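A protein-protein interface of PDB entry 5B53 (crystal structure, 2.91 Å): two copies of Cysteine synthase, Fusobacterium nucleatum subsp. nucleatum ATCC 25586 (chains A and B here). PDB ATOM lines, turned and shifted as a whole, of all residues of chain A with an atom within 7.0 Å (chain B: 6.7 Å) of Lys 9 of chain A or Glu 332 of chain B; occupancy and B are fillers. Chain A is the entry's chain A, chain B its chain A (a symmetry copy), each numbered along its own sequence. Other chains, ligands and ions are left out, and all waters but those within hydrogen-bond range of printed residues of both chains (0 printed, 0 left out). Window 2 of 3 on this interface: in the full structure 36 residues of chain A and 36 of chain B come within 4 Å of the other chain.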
ATOM      1  N   GLU A   6     -13.818  -5.750  19.522  1.00  0.00           N
ATOM      2  CA  GLU A   6     -14.901  -5.559  18.489  1.00  0.00           C
ATOM      3  C   GLU A   6     -14.416  -5.450  17.036  1.00  0.00           C
ATOM      4  O   GLU A   6     -15.078  -5.920  16.114  1.00  0.00           O
ATOM      5  CB  GLU A   6     -15.717  -4.313  18.799  1.00  0.00           C
ATOM      6  CG  GLU A   6     -16.558  -4.436  20.046  1.00  0.00           C
ATOM      7  CD  GLU A   6     -17.243  -3.128  20.358  1.00  0.00           C
ATOM      8  OE1 GLU A   6     -16.534  -2.176  20.761  1.00  0.00           O
ATOM      9  OE2 GLU A   6     -18.477  -3.061  20.177  1.00  0.00           O
ATOM     10  N   GLN A   7     -13.293  -4.771  16.835  1.00  0.00           N
ATOM     11  CA  GLN A   7     -12.542  -4.866  15.578  1.00  0.00           C
ATOM     12  C   GLN A   7     -11.779  -6.204  15.602  1.00  0.00           C
ATOM     13  O   GLN A   7     -11.347  -6.701  14.566  1.00  0.00           O
ATOM     14  CB  GLN A   7     -11.596  -3.651  15.378  1.00  0.00           C
ATOM     15  CG  GLN A   7     -12.333  -2.302  15.273  1.00  0.00           C
ATOM     16  CD  GLN A   7     -11.421  -1.086  15.113  1.00  0.00           C
ATOM     17  OE1 GLN A   7     -11.402  -0.431  14.059  1.00  0.00           O
ATOM     18  NE2 GLN A   7     -10.678  -0.766  16.168  1.00  0.00           N
ATOM     19  N   LYS A   8     -11.623  -6.770  16.799  1.00  0.00           N
ATOM     20  CA  LYS A   8     -11.193  -8.153  16.974  1.00  0.00           C
ATOM     21  C   LYS A   8     -12.267  -9.108  16.453  1.00  0.00           C
ATOM     22  O   LYS A   8     -11.937 -10.046  15.738  1.00  0.00           O
ATOM     23  CB  LYS A   8     -10.902  -8.439  18.456  1.00  0.00           C
ATOM     24  CG  LYS A   8      -9.869  -7.506  19.109  1.00  0.00           C
ATOM     25  CD  LYS A   8      -9.215  -8.140  20.341  1.00  0.00           C
ATOM     26  CE  LYS A   8      -8.072  -9.086  19.950  1.00  0.00           C
ATOM     27  NZ  LYS A   8      -7.722 -10.050  21.028  1.00  0.00           N
ATOM     28  N   LYS A   9     -13.536  -8.846  16.799  1.00  0.00           N
ATOM     29  CA  LYS A   9     -14.708  -9.687  16.409  1.00  0.00           C
ATOM     30  C   LYS A   9     -14.968  -9.598  14.953  1.00  0.00           C
ATOM     31  O   LYS A   9     -15.055 -10.579  14.271  1.00  0.00           O
ATOM     32  CB  LYS A   9     -16.008  -9.246  17.111  1.00  0.00           C
ATOM     33  CG  LYS A   9     -17.100 -10.318  17.150  1.00  0.00           C
ATOM     34  CD  LYS A   9     -18.400  -9.861  17.820  1.00  0.00           C
ATOM     35  CE  LYS A   9     -19.209 -11.086  18.290  1.00  0.00           C
ATOM     36  NZ  LYS A   9     -20.553 -10.807  18.911  1.00  0.00           N
ATOM     37  N   MET A  10     -15.113  -8.384  14.485  1.00  0.00           N
ATOM     38  CA  MET A  10     -15.258  -8.133  13.065  1.00  0.00           C
ATOM     39  C   MET A  10     -14.083  -8.717  12.282  1.00  0.00           C
ATOM     40  O   MET A  10     -14.219  -9.073  11.106  1.00  0.00           O
ATOM     41  CB  MET A  10     -15.369  -6.618  12.804  1.00  0.00           C
ATOM     42  CG  MET A  10     -16.576  -6.220  11.982  1.00  0.00           C
ATOM     43  SD  MET A  10     -18.162  -6.931  12.504  1.00  0.00           S
ATOM     44  CE  MET A  10     -18.140  -6.652  14.271  1.00  0.00           C
ATOM     45  N   LYS A  11     -12.924  -8.811  12.911  1.00  0.00           N
ATOM     46  CA  LYS A  11     -11.784  -9.335  12.185  1.00  0.00           C
ATOM     47  C   LYS A  11     -11.890 -10.859  12.069  1.00  0.00           C
ATOM     48  O   LYS A  11     -11.611 -11.399  11.006  1.00  0.00           O
ATOM     49  CB  LYS A  11     -10.443  -8.900  12.819  1.00  0.00           C
ATOM     50  CG  LYS A  11      -9.230  -8.913  11.881  1.00  0.00           C
ATOM     51  CD  LYS A  11      -7.897  -8.879  12.649  1.00  0.00           C
ATOM     52  CE  LYS A  11      -7.610 -10.191  13.401  1.00  0.00           C
ATOM     53  NZ  LYS A  11      -6.186 -10.269  13.842  1.00  0.00           N
ATOM     54  N   TYR A  12     -12.288 -11.552  13.129  1.00  0.00           N
ATOM     55  CA  TYR A  12     -12.203 -12.992  13.081  1.00  0.00           C
ATOM     56  C   TYR A  12     -13.363 -13.608  12.297  1.00  0.00           C
ATOM     57  O   TYR A  12     -13.265 -14.693  11.698  1.00  0.00           O
ATOM     58  CB  TYR A  12     -12.024 -13.614  14.484  1.00  0.00           C
ATOM     59  CG  TYR A  12     -13.091 -13.407  15.542  1.00  0.00           C
ATOM     60  CD1 TYR A  12     -14.430 -13.811  15.358  1.00  0.00           C
ATOM     61  CD2 TYR A  12     -12.727 -12.898  16.791  1.00  0.00           C
ATOM     62  CE1 TYR A  12     -15.367 -13.635  16.369  1.00  0.00           C
ATOM     63  CE2 TYR A  12     -13.652 -12.703  17.799  1.00  0.00           C
ATOM     64  CZ  TYR A  12     -14.958 -13.062  17.599  1.00  0.00           C
ATOM     65  OH  TYR A  12     -15.818 -12.858  18.654  1.00  0.00           O
ATOM     66  N   LEU A  13     -14.470 -12.898  12.275  1.00  0.00           N
ATOM     67  CA  LEU A  13     -15.622 -13.397  11.602  1.00  0.00           C
ATOM     68  C   LEU A  13     -15.394 -13.333  10.096  1.00  0.00           C
ATOM     69  O   LEU A  13     -16.088 -14.067   9.388  1.00  0.00           O
ATOM     70  CB  LEU A  13     -16.883 -12.609  12.002  1.00  0.00           C
ATOM     71  CG  LEU A  13     -17.435 -12.656  13.444  1.00  0.00           C
ATOM     72  CD1 LEU A  13     -18.578 -11.670  13.577  1.00  0.00           C
ATOM     73  CD2 LEU A  13     -17.964 -14.005  13.839  1.00  0.00           C
ATOM     74  N   GLU A  14     -14.454 -12.513   9.575  1.00  0.00           N
ATOM     75  CA  GLU A  14     -14.187 -12.637   8.152  1.00  0.00           C
ATOM     76  C   GLU A  14     -13.914 -14.092   7.853  1.00  0.00           C
ATOM     77  O   GLU A  14     -14.140 -14.536   6.738  1.00  0.00           O
ATOM     78  CB  GLU A  14     -13.220 -11.605   7.447  1.00  0.00           C
ATOM     79  CG  GLU A  14     -11.788 -11.294   7.913  1.00  0.00           C
ATOM     80  CD  GLU A  14     -11.406  -9.776   7.797  1.00  0.00           C
ATOM     81  OE1 GLU A  14     -12.314  -8.905   7.951  1.00  0.00           O
ATOM     82  OE2 GLU A  14     -10.195  -9.410   7.604  1.00  0.00           O
ATOM     83  N   PHE A  55     -21.951  -9.707   5.480  1.00  0.00           N
ATOM     84  CA  PHE A  55     -20.950  -9.514   6.483  1.00  0.00           C
ATOM     85  C   PHE A  55     -20.346  -8.172   6.208  1.00  0.00           C
ATOM     86  O   PHE A  55     -20.304  -7.311   7.045  1.00  0.00           O
ATOM     87  CB  PHE A  55     -19.865 -10.566   6.442  1.00  0.00           C
ATOM     88  CG  PHE A  55     -18.747 -10.229   7.336  1.00  0.00           C
ATOM     89  CD1 PHE A  55     -18.948 -10.243   8.715  1.00  0.00           C
ATOM     90  CD2 PHE A  55     -17.530  -9.765   6.811  1.00  0.00           C
ATOM     91  CE1 PHE A  55     -17.920  -9.860   9.576  1.00  0.00           C
ATOM     92  CE2 PHE A  55     -16.484  -9.399   7.649  1.00  0.00           C
ATOM     93  CZ  PHE A  55     -16.668  -9.460   9.039  1.00  0.00           C
ATOM     94  N   ALA A  90     -27.943 -12.216  13.753  1.00  0.00           N
ATOM     95  CA  ALA A  90     -28.049 -12.881  15.020  1.00  0.00           C
ATOM     96  C   ALA A  90     -26.686 -13.011  15.673  1.00  0.00           C
ATOM     97  O   ALA A  90     -26.534 -12.885  16.893  1.00  0.00           O
ATOM     98  CB  ALA A  90     -28.658 -14.236  14.810  1.00  0.00           C
ATOM     99  N   ILE A  91     -25.685 -13.268  14.845  1.00  0.00           N
ATOM    100  CA  ILE A  91     -24.333 -13.417  15.337  1.00  0.00           C
ATOM    101  C   ILE A  91     -23.882 -12.133  16.011  1.00  0.00           C
ATOM    102  O   ILE A  91     -23.098 -12.165  16.983  1.00  0.00           O
ATOM    103  CB  ILE A  91     -23.343 -13.716  14.197  1.00  0.00           C
ATOM    104  CG1 ILE A  91     -23.653 -15.074  13.614  1.00  0.00           C
ATOM    105  CG2 ILE A  91     -21.912 -13.616  14.718  1.00  0.00           C
ATOM    106  CD1 ILE A  91     -22.494 -15.836  13.039  1.00  0.00           C
ATOM    107  N   LEU A  92     -24.335 -11.020  15.428  1.00  0.00           N
ATOM    108  CA  LEU A  92     -24.001  -9.699  15.909  1.00  0.00           C
ATOM    109  C   LEU A  92     -25.083  -9.120  16.844  1.00  0.00           C
ATOM    110  O   LEU A  92     -25.058  -7.944  17.188  1.00  0.00           O
ATOM    111  CB  LEU A  92     -23.836  -8.808  14.685  1.00  0.00           C
ATOM    112  CG  LEU A  92     -22.552  -9.045  13.882  1.00  0.00           C
ATOM    113  CD1 LEU A  92     -22.569  -8.308  12.571  1.00  0.00           C
ATOM    114  CD2 LEU A  92     -21.300  -8.643  14.644  1.00  0.00           C
ATOM    115  N   GLY A  93     -26.067  -9.947  17.200  1.00  0.00           N
ATOM    116  CA  GLY A  93     -27.137  -9.578  18.152  1.00  0.00           C
ATOM    117  C   GLY A  93     -28.251  -8.613  17.760  1.00  0.00           C
ATOM    118  O   GLY A  93     -28.879  -8.022  18.620  1.00  0.00           O
ATOM    119  N   GLU B  24     -15.143 -20.849  18.548  1.00  0.00           N
ATOM    120  CA  GLU B  24     -15.325 -20.832  19.995  1.00  0.00           C
ATOM    121  C   GLU B  24     -16.694 -20.255  20.350  1.00  0.00           C
ATOM    122  O   GLU B  24     -16.951 -19.083  20.098  1.00  0.00           O
ATOM    123  CB  GLU B  24     -14.244 -19.979  20.636  1.00  0.00           C
ATOM    124  CG  GLU B  24     -14.295 -19.950  22.145  1.00  0.00           C
ATOM    125  CD  GLU B  24     -13.256 -19.053  22.731  1.00  0.00           C
ATOM    126  OE1 GLU B  24     -12.528 -18.432  21.915  1.00  0.00           O
ATOM    127  OE2 GLU B  24     -13.186 -18.989  23.995  1.00  0.00           O
ATOM    128  N   LEU B  25     -17.557 -21.096  20.912  1.00  0.00           N
ATOM    129  CA  LEU B  25     -18.882 -20.696  21.355  1.00  0.00           C
ATOM    130  C   LEU B  25     -18.934 -20.612  22.866  1.00  0.00           C
ATOM    131  O   LEU B  25     -18.575 -21.568  23.544  1.00  0.00           O
ATOM    132  CB  LEU B  25     -19.933 -21.716  20.920  1.00  0.00           C
ATOM    133  CG  LEU B  25     -20.082 -21.945  19.422  1.00  0.00           C
ATOM    134  CD1 LEU B  25     -21.408 -22.577  19.150  1.00  0.00           C
ATOM    135  CD2 LEU B  25     -20.035 -20.663  18.640  1.00  0.00           C
ATOM    136  N   ILE B  26     -19.443 -19.472  23.352  1.00  0.00           N
ATOM    137  CA  ILE B  26     -19.543 -19.150  24.750  1.00  0.00           C
ATOM    138  C   ILE B  26     -20.971 -19.154  25.052  1.00  0.00           C
ATOM    139  O   ILE B  26     -21.740 -18.566  24.297  1.00  0.00           O
ATOM    140  CB  ILE B  26     -19.212 -17.685  25.044  1.00  0.00           C
ATOM    141  CG1 ILE B  26     -17.867 -17.297  24.457  1.00  0.00           C
ATOM    142  CG2 ILE B  26     -19.258 -17.435  26.557  1.00  0.00           C
ATOM    143  CD1 ILE B  26     -16.728 -17.881  25.252  1.00  0.00           C
ATOM    144  N   PHE B  27     -21.330 -19.699  26.207  1.00  0.00           N
ATOM    145  CA  PHE B  27     -22.719 -19.752  26.573  1.00  0.00           C
ATOM    146  C   PHE B  27     -22.883 -19.715  28.037  1.00  0.00           C
ATOM    147  O   PHE B  27     -21.921 -19.750  28.795  1.00  0.00           O
ATOM    148  CB  PHE B  27     -23.349 -21.017  25.997  1.00  0.00           C
ATOM    149  CG  PHE B  27     -22.684 -22.283  26.420  1.00  0.00           C
ATOM    150  CD1 PHE B  27     -21.524 -22.712  25.783  1.00  0.00           C
ATOM    151  CD2 PHE B  27     -23.222 -23.061  27.447  1.00  0.00           C
ATOM    152  CE1 PHE B  27     -20.904 -23.890  26.171  1.00  0.00           C
ATOM    153  CE2 PHE B  27     -22.609 -24.231  27.841  1.00  0.00           C
ATOM    154  CZ  PHE B  27     -21.456 -24.659  27.193  1.00  0.00           C
ATOM    155  N   CYS B 269     -28.806 -18.275  16.848  1.00  0.00           N
ATOM    156  CA  CYS B 269     -27.642 -17.435  17.084  1.00  0.00           C
ATOM    157  C   CYS B 269     -26.693 -17.416  15.832  1.00  0.00           C
ATOM    158  O   CYS B 269     -25.565 -16.904  15.863  1.00  0.00           O
ATOM    159  CB  CYS B 269     -26.923 -17.849  18.368  1.00  0.00           C
ATOM    160  SG  CYS B 269     -25.434 -18.788  17.961  1.00  0.00           S
ATOM    161  N   THR B 329     -27.905 -20.811  27.526  1.00  0.00           N
ATOM    162  CA  THR B 329     -28.134 -19.601  26.754  1.00  0.00           C
ATOM    163  C   THR B 329     -26.889 -19.262  25.990  1.00  0.00           C
ATOM    164  O   THR B 329     -25.873 -19.032  26.627  1.00  0.00           O
ATOM    165  CB  THR B 329     -28.489 -18.400  27.643  1.00  0.00           C
ATOM    166  OG1 THR B 329     -29.429 -18.792  28.655  1.00  0.00           O
ATOM    167  CG2 THR B 329     -29.077 -17.297  26.770  1.00  0.00           C
ATOM    168  N   LEU B 330     -26.959 -19.210  24.653  1.00  0.00           N
ATOM    169  CA  LEU B 330     -25.766 -18.859  23.832  1.00  0.00           C
ATOM    170  C   LEU B 330     -25.498 -17.381  23.908  1.00  0.00           C
ATOM    171  O   LEU B 330     -26.342 -16.621  23.515  1.00  0.00           O
ATOM    172  CB  LEU B 330     -25.923 -19.279  22.343  1.00  0.00           C
ATOM    173  CG  LEU B 330     -26.143 -20.793  22.218  1.00  0.00           C
ATOM    174  CD1 LEU B 330     -26.607 -21.312  20.876  1.00  0.00           C
ATOM    175  CD2 LEU B 330     -24.899 -21.529  22.666  1.00  0.00           C
ATOM    176  N   LYS B 331     -24.348 -16.959  24.396  1.00  0.00           N
ATOM    177  CA  LYS B 331     -24.038 -15.535  24.304  1.00  0.00           C
ATOM    178  C   LYS B 331     -23.377 -15.125  22.941  1.00  0.00           C
ATOM    179  O   LYS B 331     -23.911 -14.319  22.204  1.00  0.00           O
ATOM    180  CB  LYS B 331     -23.139 -15.099  25.436  1.00  0.00           C
ATOM    181  CG  LYS B 331     -23.525 -15.551  26.828  1.00  0.00           C
ATOM    182  CD  LYS B 331     -22.204 -15.600  27.619  1.00  0.00           C
ATOM    183  CE  LYS B 331     -22.156 -14.710  28.872  1.00  0.00           C
ATOM    184  NZ  LYS B 331     -22.570 -15.504  30.075  1.00  0.00           N
ATOM    185  N   GLU B 332     -22.207 -15.648  22.605  1.00  0.00           N
ATOM    186  CA  GLU B 332     -21.551 -15.244  21.374  1.00  0.00           C
ATOM    187  C   GLU B 332     -20.510 -16.210  20.846  1.00  0.00           C
ATOM    188  O   GLU B 332     -20.102 -17.175  21.494  1.00  0.00           O
ATOM    189  CB  GLU B 332     -20.856 -13.914  21.583  1.00  0.00           C
ATOM    190  CG  GLU B 332     -19.766 -13.954  22.654  1.00  0.00           C
ATOM    191  CD  GLU B 332     -18.868 -12.719  22.601  1.00  0.00           C
ATOM    192  OE1 GLU B 332     -19.045 -11.912  21.663  1.00  0.00           O
ATOM    193  OE2 GLU B 332     -17.984 -12.553  23.485  1.00  0.00           O
ATOM    194  N   ILE B 333     -20.097 -15.888  19.638  1.00  0.00           N
ATOM    195  CA  ILE B 333     -19.006 -16.504  18.971  1.00  0.00           C
ATOM    196  C   ILE B 333     -17.777 -15.696  19.321  1.00  0.00           C
ATOM    197  O   ILE B 333     -17.571 -14.587  18.832  1.00  0.00           O
ATOM    198  CB  ILE B 333     -19.276 -16.428  17.484  1.00  0.00           C
ATOM    199  CG1 ILE B 333     -20.395 -17.380  17.175  1.00  0.00           C
ATOM    200  CG2 ILE B 333     -18.052 -16.798  16.696  1.00  0.00           C
ATOM    201  CD1 ILE B 333     -20.978 -17.150  15.819  1.00  0.00           C
ATOM    202  N   LYS B 334     -16.956 -16.250  20.176  1.00  0.00           N
ATOM    203  CA  LYS B 334     -15.851 -15.489  20.739  1.00  0.00           C
ATOM    204  C   LYS B 334     -14.663 -15.501  19.813  1.00  0.00           C
ATOM    205  O   LYS B 334     -13.815 -14.659  19.923  1.00  0.00           O
ATOM    206  CB  LYS B 334     -15.459 -16.040  22.135  1.00  0.00           C
ATOM    207  CG  LYS B 334     -14.343 -15.295  22.864  1.00  0.00           C
ATOM    208  CD  LYS B 334     -14.755 -13.887  23.281  1.00  0.00           C
ATOM    209  CE  LYS B 334     -13.601 -13.076  23.872  1.00  0.00           C
ATOM    210  NZ  LYS B 334     -12.919 -13.824  24.969  1.00  0.00           N
ATOM    211  N   ASN B 335     -14.606 -16.462  18.910  1.00  0.00           N
ATOM    212  CA  ASN B 335     -13.474 -16.611  18.038  1.00  0.00           C
ATOM    213  C   ASN B 335     -13.812 -17.532  16.870  1.00  0.00           C
ATOM    214  O   ASN B 335     -14.697 -18.389  17.001  1.00  0.00           O
ATOM    215  CB  ASN B 335     -12.369 -17.231  18.824  1.00  0.00           C
ATOM    216  CG  ASN B 335     -11.015 -16.886  18.289  1.00  0.00           C
ATOM    217  OD1 ASN B 335     -10.857 -16.376  17.178  1.00  0.00           O
ATOM    218  ND2 ASN B 335     -10.005 -17.160  19.097  1.00  0.00           N
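Of the 12 printed residues of chain B, 5 touch a printed residue of chain A. Hydrophobic or aromatic side chains of chain A within 4 Å of the printed part of chain B: Tyr 12, Leu 13, Ala 90 and Ile 91. Among the printed residues, 9 pairs touch across the chains. Among the printed residues, Asp or Glu carboxylates within 4 Å of a Lys or Arg side-chain nitrogen of the other chain: Lys 9 of chain A with Glu 332 of chain B (3.3 Å).
The side-chain amino group (NZ) of Lys 9 of chain A sits at hydrogen-bond distance from the backbone carbonyl oxygen (O) of Ile 91 of chain A, 3.5 Å away. N of Lys 334 of chain B lies within hydrogen-bond range of O of Glu 24 of chain B (2.8 Å). The backbone NH (N) of Glu 24 of chain B lies within hydrogen-bond range of the backbone carbonyl oxygen (O) of Asn 335 of chain B, 2.9 Å away. N of Ile 26 of chain B sits at hydrogen-bond distance from O of Glu 332 of chain B (3.0 Å).
Lys 9 of chain A touches Ile 333 of chain B (CE to O, 3.9 Å). CZ of Tyr 12 of chain A touches N of Asn 335 of chain B, 3.7 Å away. CD2 of Leu 13 of chain A touches CG2 of Ile 333 of chain B (3.996 Å). Ala 90 of chain A touches Cys 269 of chain B (CB to C, 3.9 Å). CG1 of Ile 91 of chain A touches O of Cys 269 of chain B, 3.5 Å away. CD1 of Ile 91 of chain A touches CD1 of Ile 333 of chain B, 3.4 Å away.
No position is printed for both chains.
Glu 332 of chain B touches one residue of chain A. Of the printed residues of chain A, Ile 333 of chain B touches Lys 9 (3.9 Å), Tyr 12 (2.5 Å), Leu 13 (3.996 Å) and Ile 91 (3.4 Å). Of the printed residues of chain A, Asn 335 of chain B touches Tyr 12 (3.7 Å). The nearest residue of chain B that does not touch Lys 9 of chain A is Lys 331 of chain B (5.9 Å). The nearest residue of chain A that does not touch Glu 332 of chain B is Tyr 12 of chain A (4.5 Å).
NZ of Lys 9 of chain A is in salt-bridge range of OE1 of Glu 332 of chain B (3.3 Å). The backbone carbonyl oxygen (O) of Ile 333 of chain B sits at hydrogen-bond distance from the side-chain hydroxyl (OH) of Tyr 12 of chain A (2.5 Å). OH of Tyr 12 of chain A sits close to O of Lys 334 of chain B (3.0 Å).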
